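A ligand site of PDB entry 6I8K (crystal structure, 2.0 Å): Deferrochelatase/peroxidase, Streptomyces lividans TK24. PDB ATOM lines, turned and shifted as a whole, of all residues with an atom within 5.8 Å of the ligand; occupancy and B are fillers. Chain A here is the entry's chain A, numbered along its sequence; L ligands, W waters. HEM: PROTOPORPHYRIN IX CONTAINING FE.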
ATOM      1  N   ASN A 179      20.873  20.437  -8.737  1.00  0.00           N
ATOM      2  CA  ASN A 179      19.987  20.818  -7.647  1.00  0.00           C
ATOM      3  C   ASN A 179      18.942  19.732  -7.393  1.00  0.00           C
ATOM      4  O   ASN A 179      18.940  18.669  -8.018  1.00  0.00           O
ATOM      5  CB  ASN A 179      19.317  22.159  -7.938  1.00  0.00           C
ATOM      6  CG  ASN A 179      18.670  22.200  -9.296  1.00  0.00           C
ATOM      7  OD1 ASN A 179      17.929  21.288  -9.683  1.00  0.00           O
ATOM      8  ND2 ASN A 179      18.938  23.263 -10.039  1.00  0.00           N
ATOM      9  N   LEU A 181      15.906  19.631  -8.110  1.00  0.00           N
ATOM     10  CA  LEU A 181      15.036  19.411  -9.253  1.00  0.00           C
ATOM     11  C   LEU A 181      15.637  18.494 -10.307  1.00  0.00           C
ATOM     12  O   LEU A 181      15.015  18.275 -11.356  1.00  0.00           O
ATOM     13  CB  LEU A 181      14.685  20.763  -9.904  1.00  0.00           C
ATOM     14  CG  LEU A 181      13.993  21.785  -8.997  1.00  0.00           C
ATOM     15  CD1 LEU A 181      13.485  23.023  -9.790  1.00  0.00           C
ATOM     16  CD2 LEU A 181      12.863  21.121  -8.251  1.00  0.00           C
ATOM     17  N   PHE A 183      18.392  19.019 -12.191  1.00  0.00           N
ATOM     18  CA  PHE A 183      19.096  19.628 -13.308  1.00  0.00           C
ATOM     19  C   PHE A 183      20.488  20.082 -12.879  1.00  0.00           C
ATOM     20  O   PHE A 183      20.713  20.460 -11.720  1.00  0.00           O
ATOM     21  CB  PHE A 183      18.299  20.807 -13.888  1.00  0.00           C
ATOM     22  CG  PHE A 183      17.152  20.391 -14.770  1.00  0.00           C
ATOM     23  CD1 PHE A 183      15.998  19.801 -14.225  1.00  0.00           C
ATOM     24  CD2 PHE A 183      17.208  20.552 -16.149  1.00  0.00           C
ATOM     25  CE1 PHE A 183      14.941  19.404 -15.024  1.00  0.00           C
ATOM     26  CE2 PHE A 183      16.151  20.151 -16.965  1.00  0.00           C
ATOM     27  CZ  PHE A 183      15.010  19.570 -16.404  1.00  0.00           C
ATOM     28  N   LYS A 184      21.447  20.015 -13.805  1.00  0.00           N
ATOM     29  CA  LYS A 184      22.759  20.616 -13.562  1.00  0.00           C
ATOM     30  C   LYS A 184      22.574  22.105 -13.340  1.00  0.00           C
ATOM     31  O   LYS A 184      21.834  22.766 -14.073  1.00  0.00           O
ATOM     32  CB  LYS A 184      23.721  20.378 -14.734  1.00  0.00           C
ATOM     33  CG  LYS A 184      23.909  18.927 -15.142  1.00  0.00           C
ATOM     34  CD  LYS A 184      24.814  18.851 -16.389  1.00  0.00           C
ATOM     35  CE  LYS A 184      25.353  17.439 -16.622  1.00  0.00           C
ATOM     36  NZ  LYS A 184      26.085  17.355 -17.936  1.00  0.00           N
ATOM     37  N   ASP A 185      23.244  22.633 -12.324  1.00  0.00           N
ATOM     38  CA  ASP A 185      23.085  24.026 -11.907  1.00  0.00           C
ATOM     39  C   ASP A 185      24.465  24.646 -11.813  1.00  0.00           C
ATOM     40  O   ASP A 185      25.277  24.225 -10.989  1.00  0.00           O
ATOM     41  CB  ASP A 185      22.354  24.111 -10.553  1.00  0.00           C
ATOM     42  CG  ASP A 185      21.625  25.442 -10.328  1.00  0.00           C
ATOM     43  OD1 ASP A 185      22.008  26.497 -10.899  1.00  0.00           O
ATOM     44  OD2 ASP A 185      20.629  25.437  -9.577  1.00  0.00           O
ATOM     45  N   GLY A 186      24.731  25.650 -12.656  1.00  0.00           N
ATOM     46  CA  GLY A 186      26.002  26.347 -12.615  1.00  0.00           C
ATOM     47  C   GLY A 186      26.835  26.286 -13.887  1.00  0.00           C
ATOM     48  O   GLY A 186      27.987  26.716 -13.885  1.00  0.00           O
ATOM     49  N   THR A 187      26.256  25.805 -14.986  1.00  0.00           N
ATOM     50  CA  THR A 187      26.996  25.660 -16.244  1.00  0.00           C
ATOM     51  C   THR A 187      27.524  27.001 -16.718  1.00  0.00           C
ATOM     52  O   THR A 187      28.733  27.187 -16.907  1.00  0.00           O
ATOM     53  CB  THR A 187      26.095  25.021 -17.288  1.00  0.00           C
ATOM     54  OG1 THR A 187      25.707  23.715 -16.833  1.00  0.00           O
ATOM     55  CG2 THR A 187      26.786  24.904 -18.637  1.00  0.00           C
ATOM     56  N   ARG A 188      26.629  27.969 -16.911  1.00  0.00           N
ATOM     57  CA  ARG A 188      27.020  29.302 -17.372  1.00  0.00           C
ATOM     58  C   ARG A 188      27.046  30.250 -16.175  1.00  0.00           C
ATOM     59  O   ARG A 188      26.130  31.051 -15.953  1.00  0.00           O
ATOM     60  CB  ARG A 188      26.091  29.769 -18.485  1.00  0.00           C
ATOM     61  CG  ARG A 188      26.358  29.046 -19.807  1.00  0.00           C
ATOM     62  CD  ARG A 188      25.608  29.675 -20.977  1.00  0.00           C
ATOM     63  NE  ARG A 188      25.288  31.060 -20.686  1.00  0.00           N
ATOM     64  CZ  ARG A 188      26.096  32.082 -20.954  1.00  0.00           C
ATOM     65  NH1 ARG A 188      25.728  33.307 -20.646  1.00  0.00           N
ATOM     66  NH2 ARG A 188      27.256  31.861 -21.551  1.00  0.00           N
ATOM     67  N   ASN A 189      28.111  30.133 -15.396  1.00  0.00           N
ATOM     68  CA  ASN A 189      28.387  31.008 -14.271  1.00  0.00           C
ATOM     69  C   ASN A 189      29.659  31.792 -14.593  1.00  0.00           C
ATOM     70  O   ASN A 189      30.135  31.790 -15.730  1.00  0.00           O
ATOM     71  CB  ASN A 189      28.494  30.198 -12.979  1.00  0.00           C
ATOM     72  CG  ASN A 189      28.308  31.054 -11.748  1.00  0.00           C
ATOM     73  OD1 ASN A 189      27.606  32.047 -11.790  1.00  0.00           O
ATOM     74  ND2 ASN A 189      28.925  30.647 -10.641  1.00  0.00           N
ATOM     75  N   ILE A 224      14.755  29.897  -1.021  1.00  0.00           N
ATOM     76  CA  ILE A 224      13.766  29.561  -2.043  1.00  0.00           C
ATOM     77  C   ILE A 224      13.275  28.147  -1.818  1.00  0.00           C
ATOM     78  O   ILE A 224      14.041  27.191  -1.977  1.00  0.00           O
ATOM     79  CB  ILE A 224      14.324  29.716  -3.455  1.00  0.00           C
ATOM     80  CG1 ILE A 224      14.777  31.163  -3.678  1.00  0.00           C
ATOM     81  CG2 ILE A 224      13.267  29.295  -4.462  1.00  0.00           C
ATOM     82  CD1 ILE A 224      15.544  31.370  -4.979  1.00  0.00           C
ATOM     83  N   MET A 226      11.153  24.820  -2.816  1.00  0.00           N
ATOM     84  CA  MET A 226      10.704  24.118  -4.013  1.00  0.00           C
ATOM     85  C   MET A 226       9.485  23.239  -3.709  1.00  0.00           C
ATOM     86  O   MET A 226       9.473  22.494  -2.716  1.00  0.00           O
ATOM     87  CB  MET A 226      11.816  23.257  -4.598  1.00  0.00           C
ATOM     88  CG  MET A 226      13.088  23.997  -4.981  1.00  0.00           C
ATOM     89  SD  MET A 226      14.417  22.774  -5.057  1.00  0.00           S
ATOM     90  CE  MET A 226      15.568  23.492  -6.241  1.00  0.00           C
ATOM     91  N   PHE A 243      13.190  24.924 -18.126  1.00  0.00           N
ATOM     92  CA  PHE A 243      14.540  25.471 -18.076  1.00  0.00           C
ATOM     93  C   PHE A 243      15.063  25.887 -19.442  1.00  0.00           C
ATOM     94  O   PHE A 243      15.684  26.957 -19.565  1.00  0.00           O
ATOM     95  CB  PHE A 243      15.496  24.461 -17.431  1.00  0.00           C
ATOM     96  CG  PHE A 243      15.282  24.363 -15.961  1.00  0.00           C
ATOM     97  CD1 PHE A 243      15.647  25.413 -15.127  1.00  0.00           C
ATOM     98  CD2 PHE A 243      14.632  23.275 -15.409  1.00  0.00           C
ATOM     99  CE1 PHE A 243      15.412  25.365 -13.770  1.00  0.00           C
ATOM    100  CE2 PHE A 243      14.400  23.220 -14.045  1.00  0.00           C
ATOM    101  CZ  PHE A 243      14.794  24.273 -13.221  1.00  0.00           C
ATOM    102  N   ARG A 245      16.987  23.606 -21.045  1.00  0.00           N
ATOM    103  CA  ARG A 245      18.051  22.634 -21.198  1.00  0.00           C
ATOM    104  C   ARG A 245      17.438  21.264 -20.952  1.00  0.00           C
ATOM    105  O   ARG A 245      16.392  21.135 -20.318  1.00  0.00           O
ATOM    106  CB  ARG A 245      19.219  22.901 -20.227  1.00  0.00           C
ATOM    107  CG  ARG A 245      19.953  24.220 -20.431  1.00  0.00           C
ATOM    108  CD  ARG A 245      21.092  24.403 -19.420  1.00  0.00           C
ATOM    109  NE  ARG A 245      21.900  25.606 -19.694  1.00  0.00           N
ATOM    110  CZ  ARG A 245      23.021  25.583 -20.427  1.00  0.00           C
ATOM    111  NH1 ARG A 245      23.449  24.438 -20.939  1.00  0.00           N
ATOM    112  NH2 ARG A 245      23.714  26.705 -20.647  1.00  0.00           N
ATOM    113  N   PRO A 262      23.787  28.426 -25.581  1.00  0.00           N
ATOM    114  CA  PRO A 262      22.337  28.396 -25.824  1.00  0.00           C
ATOM    115  C   PRO A 262      21.977  29.238 -27.035  1.00  0.00           C
ATOM    116  O   PRO A 262      22.573  30.277 -27.307  1.00  0.00           O
ATOM    117  CB  PRO A 262      21.746  28.972 -24.532  1.00  0.00           C
ATOM    118  CG  PRO A 262      22.861  29.813 -23.974  1.00  0.00           C
ATOM    119  CD  PRO A 262      24.113  29.052 -24.284  1.00  0.00           C
ATOM    120  N   HIS A 272      13.407  29.532 -18.142  1.00  0.00           N
ATOM    121  CA  HIS A 272      14.270  30.131 -17.127  1.00  0.00           C
ATOM    122  C   HIS A 272      15.600  30.611 -17.714  1.00  0.00           C
ATOM    123  O   HIS A 272      16.016  31.747 -17.454  1.00  0.00           O
ATOM    124  CB  HIS A 272      14.532  29.104 -16.032  1.00  0.00           C
ATOM    125  CG  HIS A 272      15.318  29.650 -14.890  1.00  0.00           C
ATOM    126  ND1 HIS A 272      14.859  30.680 -14.092  1.00  0.00           N
ATOM    127  CD2 HIS A 272      16.549  29.325 -14.429  1.00  0.00           C
ATOM    128  CE1 HIS A 272      15.761  30.956 -13.173  1.00  0.00           C
ATOM    129  NE2 HIS A 272      16.797  30.155 -13.354  1.00  0.00           N
ATOM    130  N   VAL A 273      16.268  29.768 -18.509  1.00  0.00           N
ATOM    131  CA  VAL A 273      17.563  30.191 -19.073  1.00  0.00           C
ATOM    132  C   VAL A 273      17.380  31.369 -20.014  1.00  0.00           C
ATOM    133  O   VAL A 273      18.136  32.341 -19.978  1.00  0.00           O
ATOM    134  CB  VAL A 273      18.271  29.013 -19.760  1.00  0.00           C
ATOM    135  CG1 VAL A 273      19.452  29.515 -20.562  1.00  0.00           C
ATOM    136  CG2 VAL A 273      18.766  28.028 -18.747  1.00  0.00           C
ATOM    137  N   ALA A 276      16.826  34.505 -17.790  1.00  0.00           N
ATOM    138  CA  ALA A 276      17.951  34.817 -16.927  1.00  0.00           C
ATOM    139  C   ALA A 276      19.219  35.175 -17.692  1.00  0.00           C
ATOM    140  O   ALA A 276      20.103  35.823 -17.131  1.00  0.00           O
ATOM    141  CB  ALA A 276      18.241  33.626 -16.002  1.00  0.00           C
ATOM    142  N   HIS A 277      19.299  34.815 -18.982  1.00  0.00           N
ATOM    143  CA  HIS A 277      20.539  34.953 -19.733  1.00  0.00           C
ATOM    144  C   HIS A 277      20.921  36.426 -19.865  1.00  0.00           C
ATOM    145  O   HIS A 277      20.060  37.274 -20.059  1.00  0.00           O
ATOM    146  CB  HIS A 277      20.345  34.317 -21.122  1.00  0.00           C
ATOM    147  CG  HIS A 277      21.614  34.191 -21.907  1.00  0.00           C
ATOM    148  ND1 HIS A 277      22.172  35.241 -22.598  1.00  0.00           N
ATOM    149  CD2 HIS A 277      22.416  33.118 -22.121  1.00  0.00           C
ATOM    150  CE1 HIS A 277      23.270  34.837 -23.192  1.00  0.00           C
ATOM    151  NE2 HIS A 277      23.441  33.554 -22.921  1.00  0.00           N
ATOM    152  N   PRO A 278      22.220  36.757 -19.762  1.00  0.00           N
ATOM    153  CA  PRO A 278      22.605  38.186 -19.795  1.00  0.00           C
ATOM    154  C   PRO A 278      22.134  38.925 -21.053  1.00  0.00           C
ATOM    155  O   PRO A 278      21.845  40.121 -20.978  1.00  0.00           O
ATOM    156  CB  PRO A 278      24.134  38.145 -19.709  1.00  0.00           C
ATOM    157  CG  PRO A 278      24.432  36.863 -18.994  1.00  0.00           C
ATOM    158  CD  PRO A 278      23.371  35.888 -19.454  1.00  0.00           C
ATOM    159  N   LEU A 286      25.582  37.588 -13.073  1.00  0.00           N
ATOM    160  CA  LEU A 286      25.774  37.308 -11.654  1.00  0.00           C
ATOM    161  C   LEU A 286      26.782  36.197 -11.475  1.00  0.00           C
ATOM    162  O   LEU A 286      27.066  35.436 -12.403  1.00  0.00           O
ATOM    163  CB  LEU A 286      24.464  36.897 -10.980  1.00  0.00           C
ATOM    164  CG  LEU A 286      23.205  37.646 -11.403  1.00  0.00           C
ATOM    165  CD1 LEU A 286      21.982  36.780 -11.208  1.00  0.00           C
ATOM    166  CD2 LEU A 286      23.098  38.902 -10.538  1.00  0.00           C
ATOM    167  N   ARG A 288      26.679  33.015  -9.288  1.00  0.00           N
ATOM    168  CA  ARG A 288      25.854  32.202  -8.415  1.00  0.00           C
ATOM    169  C   ARG A 288      26.734  31.296  -7.561  1.00  0.00           C
ATOM    170  O   ARG A 288      27.785  30.826  -8.012  1.00  0.00           O
ATOM    171  CB  ARG A 288      24.854  31.400  -9.249  1.00  0.00           C
ATOM    172  CG  ARG A 288      23.752  32.284  -9.796  1.00  0.00           C
ATOM    173  CD  ARG A 288      22.921  31.578 -10.857  1.00  0.00           C
ATOM    174  NE  ARG A 288      23.700  31.327 -12.053  1.00  0.00           N
ATOM    175  CZ  ARG A 288      23.672  30.182 -12.731  1.00  0.00           C
ATOM    176  NH1 ARG A 288      22.904  29.174 -12.321  1.00  0.00           N
ATOM    177  NH2 ARG A 288      24.420  30.058 -13.827  1.00  0.00           N
ATOM    178  N   LEU A 307      16.358  25.648  -2.115  1.00  0.00           N
ATOM    179  CA  LEU A 307      17.651  26.138  -2.571  1.00  0.00           C
ATOM    180  C   LEU A 307      17.955  27.447  -1.869  1.00  0.00           C
ATOM    181  O   LEU A 307      17.153  28.388  -1.921  1.00  0.00           O
ATOM    182  CB  LEU A 307      17.657  26.338  -4.086  1.00  0.00           C
ATOM    183  CG  LEU A 307      19.028  26.663  -4.666  1.00  0.00           C
ATOM    184  CD1 LEU A 307      19.379  25.675  -5.775  1.00  0.00           C
ATOM    185  CD2 LEU A 307      19.063  28.098  -5.162  1.00  0.00           C
ATOM    186  N   PHE A 309      19.862  30.452  -2.231  1.00  0.00           N
ATOM    187  CA  PHE A 309      20.433  31.089  -3.402  1.00  0.00           C
ATOM    188  C   PHE A 309      21.296  32.277  -2.970  1.00  0.00           C
ATOM    189  O   PHE A 309      20.840  33.133  -2.204  1.00  0.00           O
ATOM    190  CB  PHE A 309      19.302  31.524  -4.345  1.00  0.00           C
ATOM    191  CG  PHE A 309      19.756  32.246  -5.601  1.00  0.00           C
ATOM    192  CD1 PHE A 309      19.958  33.621  -5.583  1.00  0.00           C
ATOM    193  CD2 PHE A 309      19.968  31.556  -6.791  1.00  0.00           C
ATOM    194  CE1 PHE A 309      20.363  34.313  -6.734  1.00  0.00           C
ATOM    195  CE2 PHE A 309      20.367  32.226  -7.943  1.00  0.00           C
ATOM    196  CZ  PHE A 309      20.570  33.619  -7.911  1.00  0.00           C
ATOM    197  N   PHE A 320      21.354  41.515  -9.464  1.00  0.00           N
ATOM    198  CA  PHE A 320      20.215  40.667  -9.157  1.00  0.00           C
ATOM    199  C   PHE A 320      18.893  41.363  -9.488  1.00  0.00           C
ATOM    200  O   PHE A 320      17.965  40.731  -9.989  1.00  0.00           O
ATOM    201  CB  PHE A 320      20.272  40.265  -7.681  1.00  0.00           C
ATOM    202  CG  PHE A 320      19.101  39.470  -7.210  1.00  0.00           C
ATOM    203  CD1 PHE A 320      19.113  38.066  -7.275  1.00  0.00           C
ATOM    204  CD2 PHE A 320      17.992  40.106  -6.657  1.00  0.00           C
ATOM    205  CE1 PHE A 320      18.016  37.314  -6.816  1.00  0.00           C
ATOM    206  CE2 PHE A 320      16.887  39.369  -6.195  1.00  0.00           C
ATOM    207  CZ  PHE A 320      16.900  37.961  -6.278  1.00  0.00           C
ATOM    208  N   VAL A 323      17.698  41.056 -13.159  1.00  0.00           N
ATOM    209  CA  VAL A 323      17.469  39.658 -13.546  1.00  0.00           C
ATOM    210  C   VAL A 323      16.263  39.087 -12.801  1.00  0.00           C
ATOM    211  O   VAL A 323      15.455  38.342 -13.378  1.00  0.00           O
ATOM    212  CB  VAL A 323      18.734  38.807 -13.313  1.00  0.00           C
ATOM    213  CG1 VAL A 323      18.512  37.379 -13.836  1.00  0.00           C
ATOM    214  CG2 VAL A 323      19.958  39.433 -13.969  1.00  0.00           C
ATOM    215  N   GLN A 324      16.131  39.405 -11.523  1.00  0.00           N
ATOM    216  CA  GLN A 324      14.934  38.958 -10.805  1.00  0.00           C
ATOM    217  C   GLN A 324      13.678  39.566 -11.410  1.00  0.00           C
ATOM    218  O   GLN A 324      12.650  38.892 -11.551  1.00  0.00           O
ATOM    219  CB  GLN A 324      15.045  39.304  -9.314  1.00  0.00           C
ATOM    220  CG  GLN A 324      13.880  38.772  -8.475  1.00  0.00           C
ATOM    221  CD  GLN A 324      13.683  37.258  -8.591  1.00  0.00           C
ATOM    222  OE1 GLN A 324      14.465  36.557  -9.229  1.00  0.00           O
ATOM    223  NE2 GLN A 324      12.647  36.746  -7.940  1.00  0.00           N
ATOM    224  N   LEU A 327      12.456  37.709 -14.315  1.00  0.00           N
ATOM    225  CA  LEU A 327      11.860  36.409 -14.008  1.00  0.00           C
ATOM    226  C   LEU A 327      10.384  36.495 -13.610  1.00  0.00           C
ATOM    227  O   LEU A 327       9.789  35.462 -13.281  1.00  0.00           O
ATOM    228  CB  LEU A 327      12.668  35.719 -12.898  1.00  0.00           C
ATOM    229  CG  LEU A 327      14.178  35.593 -13.167  1.00  0.00           C
ATOM    230  CD1 LEU A 327      14.899  34.790 -12.042  1.00  0.00           C
ATOM    231  CD2 LEU A 327      14.424  34.960 -14.517  1.00  0.00           C
ATOM    232  N   LEU A 332       9.517  28.649 -14.177  1.00  0.00           N
ATOM    233  CA  LEU A 332       9.923  28.046 -12.917  1.00  0.00           C
ATOM    234  C   LEU A 332       9.105  28.575 -11.727  1.00  0.00           C
ATOM    235  O   LEU A 332       9.017  27.894 -10.705  1.00  0.00           O
ATOM    236  CB  LEU A 332      11.404  28.316 -12.726  1.00  0.00           C
ATOM    237  CG  LEU A 332      12.099  27.781 -11.485  1.00  0.00           C
ATOM    238  CD1 LEU A 332      12.072  26.238 -11.468  1.00  0.00           C
ATOM    239  CD2 LEU A 332      13.510  28.325 -11.491  1.00  0.00           C
ATOM    240  N   ILE A 336       8.411  27.184  -7.367  1.00  0.00           N
ATOM    241  CA  ILE A 336       9.242  27.710  -6.301  1.00  0.00           C
ATOM    242  C   ILE A 336       8.530  28.850  -5.588  1.00  0.00           C
ATOM    243  O   ILE A 336       7.560  29.430  -6.083  1.00  0.00           O
ATOM    244  CB  ILE A 336      10.602  28.215  -6.828  1.00  0.00           C
ATOM    245  CG1 ILE A 336      10.400  29.518  -7.608  1.00  0.00           C
ATOM    246  CG2 ILE A 336      11.281  27.149  -7.643  1.00  0.00           C
ATOM    247  CD1 ILE A 336      11.681  30.126  -8.127  1.00  0.00           C
ATOM    248  N   HIS A 338       9.962  32.239  -3.002  1.00  0.00           N
ATOM    249  CA  HIS A 338      10.974  32.896  -2.194  1.00  0.00           C
ATOM    250  C   HIS A 338      10.411  33.178  -0.810  1.00  0.00           C
ATOM    251  O   HIS A 338       9.367  33.826  -0.666  1.00  0.00           O
ATOM    252  CB  HIS A 338      11.432  34.195  -2.845  1.00  0.00           C
ATOM    253  CG  HIS A 338      12.170  34.021  -4.138  1.00  0.00           C
ATOM    254  ND1 HIS A 338      13.376  34.633  -4.406  1.00  0.00           N
ATOM    255  CD2 HIS A 338      11.848  33.324  -5.264  1.00  0.00           C
ATOM    256  CE1 HIS A 338      13.782  34.307  -5.622  1.00  0.00           C
ATOM    257  NE2 HIS A 338      12.871  33.520  -6.159  1.00  0.00           N
HETATM  258  CHA HEM L   1      20.887  29.261 -14.920  1.00  0.00           C
HETATM  259  CHB HEM L   1      18.168  26.654 -11.897  1.00  0.00           C
HETATM  260  CHC HEM L   1      16.937  30.580  -9.347  1.00  0.00           C
HETATM  261  CHD HEM L   1      19.613  33.215 -12.450  1.00  0.00           C
HETATM  262  C1A HEM L   1      20.217  28.213 -14.354  1.00  0.00           C
HETATM  263  C2A HEM L   1      20.155  26.864 -14.856  1.00  0.00           C
HETATM  264  C3A HEM L   1      19.386  26.159 -14.030  1.00  0.00           C
HETATM  265  C4A HEM L   1      18.955  27.031 -12.951  1.00  0.00           C
HETATM  266  CMA HEM L   1      19.036  24.666 -14.170  1.00  0.00           C
HETATM  267  CAA HEM L   1      20.832  26.339 -16.144  1.00  0.00           C
HETATM  268  CBA HEM L   1      22.283  25.903 -15.907  1.00  0.00           C
HETATM  269  CGA HEM L   1      23.236  27.000 -15.492  1.00  0.00           C
HETATM  270  O1A HEM L   1      23.756  27.677 -16.408  1.00  0.00           O
HETATM  271  O2A HEM L   1      23.526  27.183 -14.274  1.00  0.00           O
HETATM  272  C1B HEM L   1      17.615  27.472 -10.943  1.00  0.00           C
HETATM  273  C2B HEM L   1      16.757  27.051  -9.853  1.00  0.00           C
HETATM  274  C3B HEM L   1      16.404  28.143  -9.159  1.00  0.00           C
HETATM  275  C4B HEM L   1      17.037  29.277  -9.776  1.00  0.00           C
HETATM  276  CMB HEM L   1      16.359  25.576  -9.609  1.00  0.00           C
HETATM  277  CAB HEM L   1      15.524  28.253  -7.882  1.00  0.00           C
HETATM  278  CBB HEM L   1      15.367  27.217  -7.044  1.00  0.00           C
HETATM  279  C1C HEM L   1      17.553  31.634  -9.965  1.00  0.00           C
HETATM  280  C2C HEM L   1      17.451  33.000  -9.581  1.00  0.00           C
HETATM  281  C3C HEM L   1      18.208  33.728 -10.437  1.00  0.00           C
HETATM  282  C4C HEM L   1      18.781  32.833 -11.409  1.00  0.00           C
HETATM  283  CMC HEM L   1      16.629  33.444  -8.348  1.00  0.00           C
HETATM  284  CAC HEM L   1      18.440  35.248 -10.481  1.00  0.00           C
HETATM  285  CBC HEM L   1      17.672  36.064  -9.744  1.00  0.00           C
HETATM  286  C1D HEM L   1      20.231  32.383 -13.350  1.00  0.00           C
HETATM  287  C2D HEM L   1      21.254  32.754 -14.308  1.00  0.00           C
HETATM  288  C3D HEM L   1      21.594  31.673 -14.988  1.00  0.00           C
HETATM  289  C4D HEM L   1      20.811  30.562 -14.490  1.00  0.00           C
HETATM  290  CMD HEM L   1      21.864  34.162 -14.549  1.00  0.00           C
HETATM  291  CAD HEM L   1      22.652  31.620 -16.108  1.00  0.00           C
HETATM  292  CBD HEM L   1      21.926  31.781 -17.444  1.00  0.00           C
HETATM  293  CGD HEM L   1      22.880  31.892 -18.618  1.00  0.00           C
HETATM  294  O1D HEM L   1      22.873  30.960 -19.474  1.00  0.00           O
HETATM  295  O2D HEM L   1      23.629  32.895 -18.702  1.00  0.00           O
HETATM  296  NA  HEM L   1      19.477  28.280 -13.185  1.00  0.00           N
HETATM  297  NB  HEM L   1      17.768  28.843 -10.867  1.00  0.00           N
HETATM  298  NC  HEM L   1      18.371  31.558 -11.081  1.00  0.00           N
HETATM  299  ND  HEM L   1      19.996  31.031 -13.470  1.00  0.00           N
HETATM  300 FE   HEM L   1      18.714  29.937 -12.230  1.00  0.00          FE
HETATM  301  O   HOH W   1      22.478  28.300 -18.741  1.00  0.00           O
HETATM  302  O   HOH W   2      22.444  37.000 -15.787  1.00  0.00           O
HETATM  303  O   HOH W   3      25.747  33.756 -17.161  1.00  0.00           O
HETATM  304  O   HOH W   4      20.531  28.769 -10.184  1.00  0.00           O
HETATM  305  O   HOH W   5      24.523  35.698 -14.931  1.00  0.00           O
HETATM  306  O   HOH W   6      13.202  33.515  -9.028  1.00  0.00           O
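Asn 179 touches the ligand (ND2 to CMB, 3.5 Å).
CD1 of Leu 181 touches CMB of the ligand, 3.8 Å away.
CB of Phe 183 touches CMA of the ligand, 3.9 Å away.
O of Lys 184 touches CMA of the ligand (3.4 Å).
Asp 185 touches the ligand.
CG2 of Ile 224 touches CBB of the ligand, 3.9 Å away.
Met 226 touches the ligand.
Phe 243 touches the ligand.
Arg 245 touches the ligand.
Val 273 touches the ligand (CG2 to CAA, 3.7 Å).
Ala 276 touches the ligand (O to CMD, 3.5 Å).
His 277 touches the ligand.
Pro 278 touches the ligand (CD to O2D, 3.1 Å).
Leu 286 touches the ligand.
CB of Leu 307 touches CBB of the ligand, at 3.8 Å.
CE2 of Phe 309 touches C2C of the ligand, 3.4 Å away.
Phe 320 touches the ligand (CE1 to CBC, 3.2 Å).
CG1 of Val 323 touches CAC of the ligand (3.98 Å).
Gln 324 touches the ligand (OE1 to CBC, 3.3 Å).
Leu 327 touches the ligand.
Leu 332 touches the ligand (CD2 to C3B, 3.7 Å).
Hydrophobic or aromatic side chains within 4 Å of the ligand: Leu 181, Phe 183, Ile 224, Met 226, Phe 243, His 272, Val 273, Ala 276, His 277, Pro 278, Leu 286, Leu 307, Phe 309, Phe 320, Val 323, Leu 327 and Leu 332.
Of the 30 residues printed, 26 come within 4 Å of the ligand.
An oxygen (O2A) of the ligand is in salt-bridge range of the guanidinium group (NH1) of Arg 288 (2.9 Å).
N of Gly 186 is in hydrogen-bond range of O2A of the ligand (2.5 Å).
N of Thr 187 is in hydrogen-bond range of O2A of the ligand.
An oxygen (O1A) of the ligand sits at hydrogen-bond distance from the backbone NH of Arg 188.
O1D of the ligand is in salt-bridge range of NE of Arg 188 (2.7 Å).
FE of the ligand is bound by NE2 of His 272, at 2.2 Å.
The backbone NH (N) of Arg 288 sits at hydrogen-bond distance from the side-chain amide oxygen (OD1) of Asn 189, 2.8 Å away.
The side-chain amide nitrogen (ND2) of Asn 179 lies within hydrogen-bond range of the side-chain carboxylate (OD2) of Asp 185 (2.8 Å).
O of Arg 188 lies within hydrogen-bond range of NH2 of Arg 288 (2.9 Å).
The backbone carbonyl oxygen (O) of Leu 286 sits close to the side-chain amide oxygen (OD1) of Asn 189.
O of Phe 243 is in hydrogen-bond range of N of Val 273, 3.1 Å away.
OD1 of Asn 179 sits at hydrogen-bond distance from N of Phe 183, 3.4 Å away.
NH1 of Arg 288 lies within salt-bridge range of OD1 of Asp 185 (3.2 Å).
The side-chain amide oxygen (OD1) of Asn 179 is in hydrogen-bond range of the backbone NH (N) of Leu 181 (3.1 Å).
Water W1 bridges an oxygen (O1A) of the ligand (2.7 Å) and the guanidinium group of Arg 245 (2.8 Å).
Water W3 lies within hydrogen-bond range of an oxygen (O2D) of the ligand (2.8 Å) and the backbone carbonyl oxygen (O) of Arg 188 (3.0 Å).
Water W4 lies within hydrogen-bond range of the side-chain carboxylate of Asp 185 (2.8 Å) and the guanidinium group of Arg 288 (3.2 Å).
Water W6 bridges NE2 of His 338 (2.9 Å) and OE1 of Gln 324 (3.3 Å).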
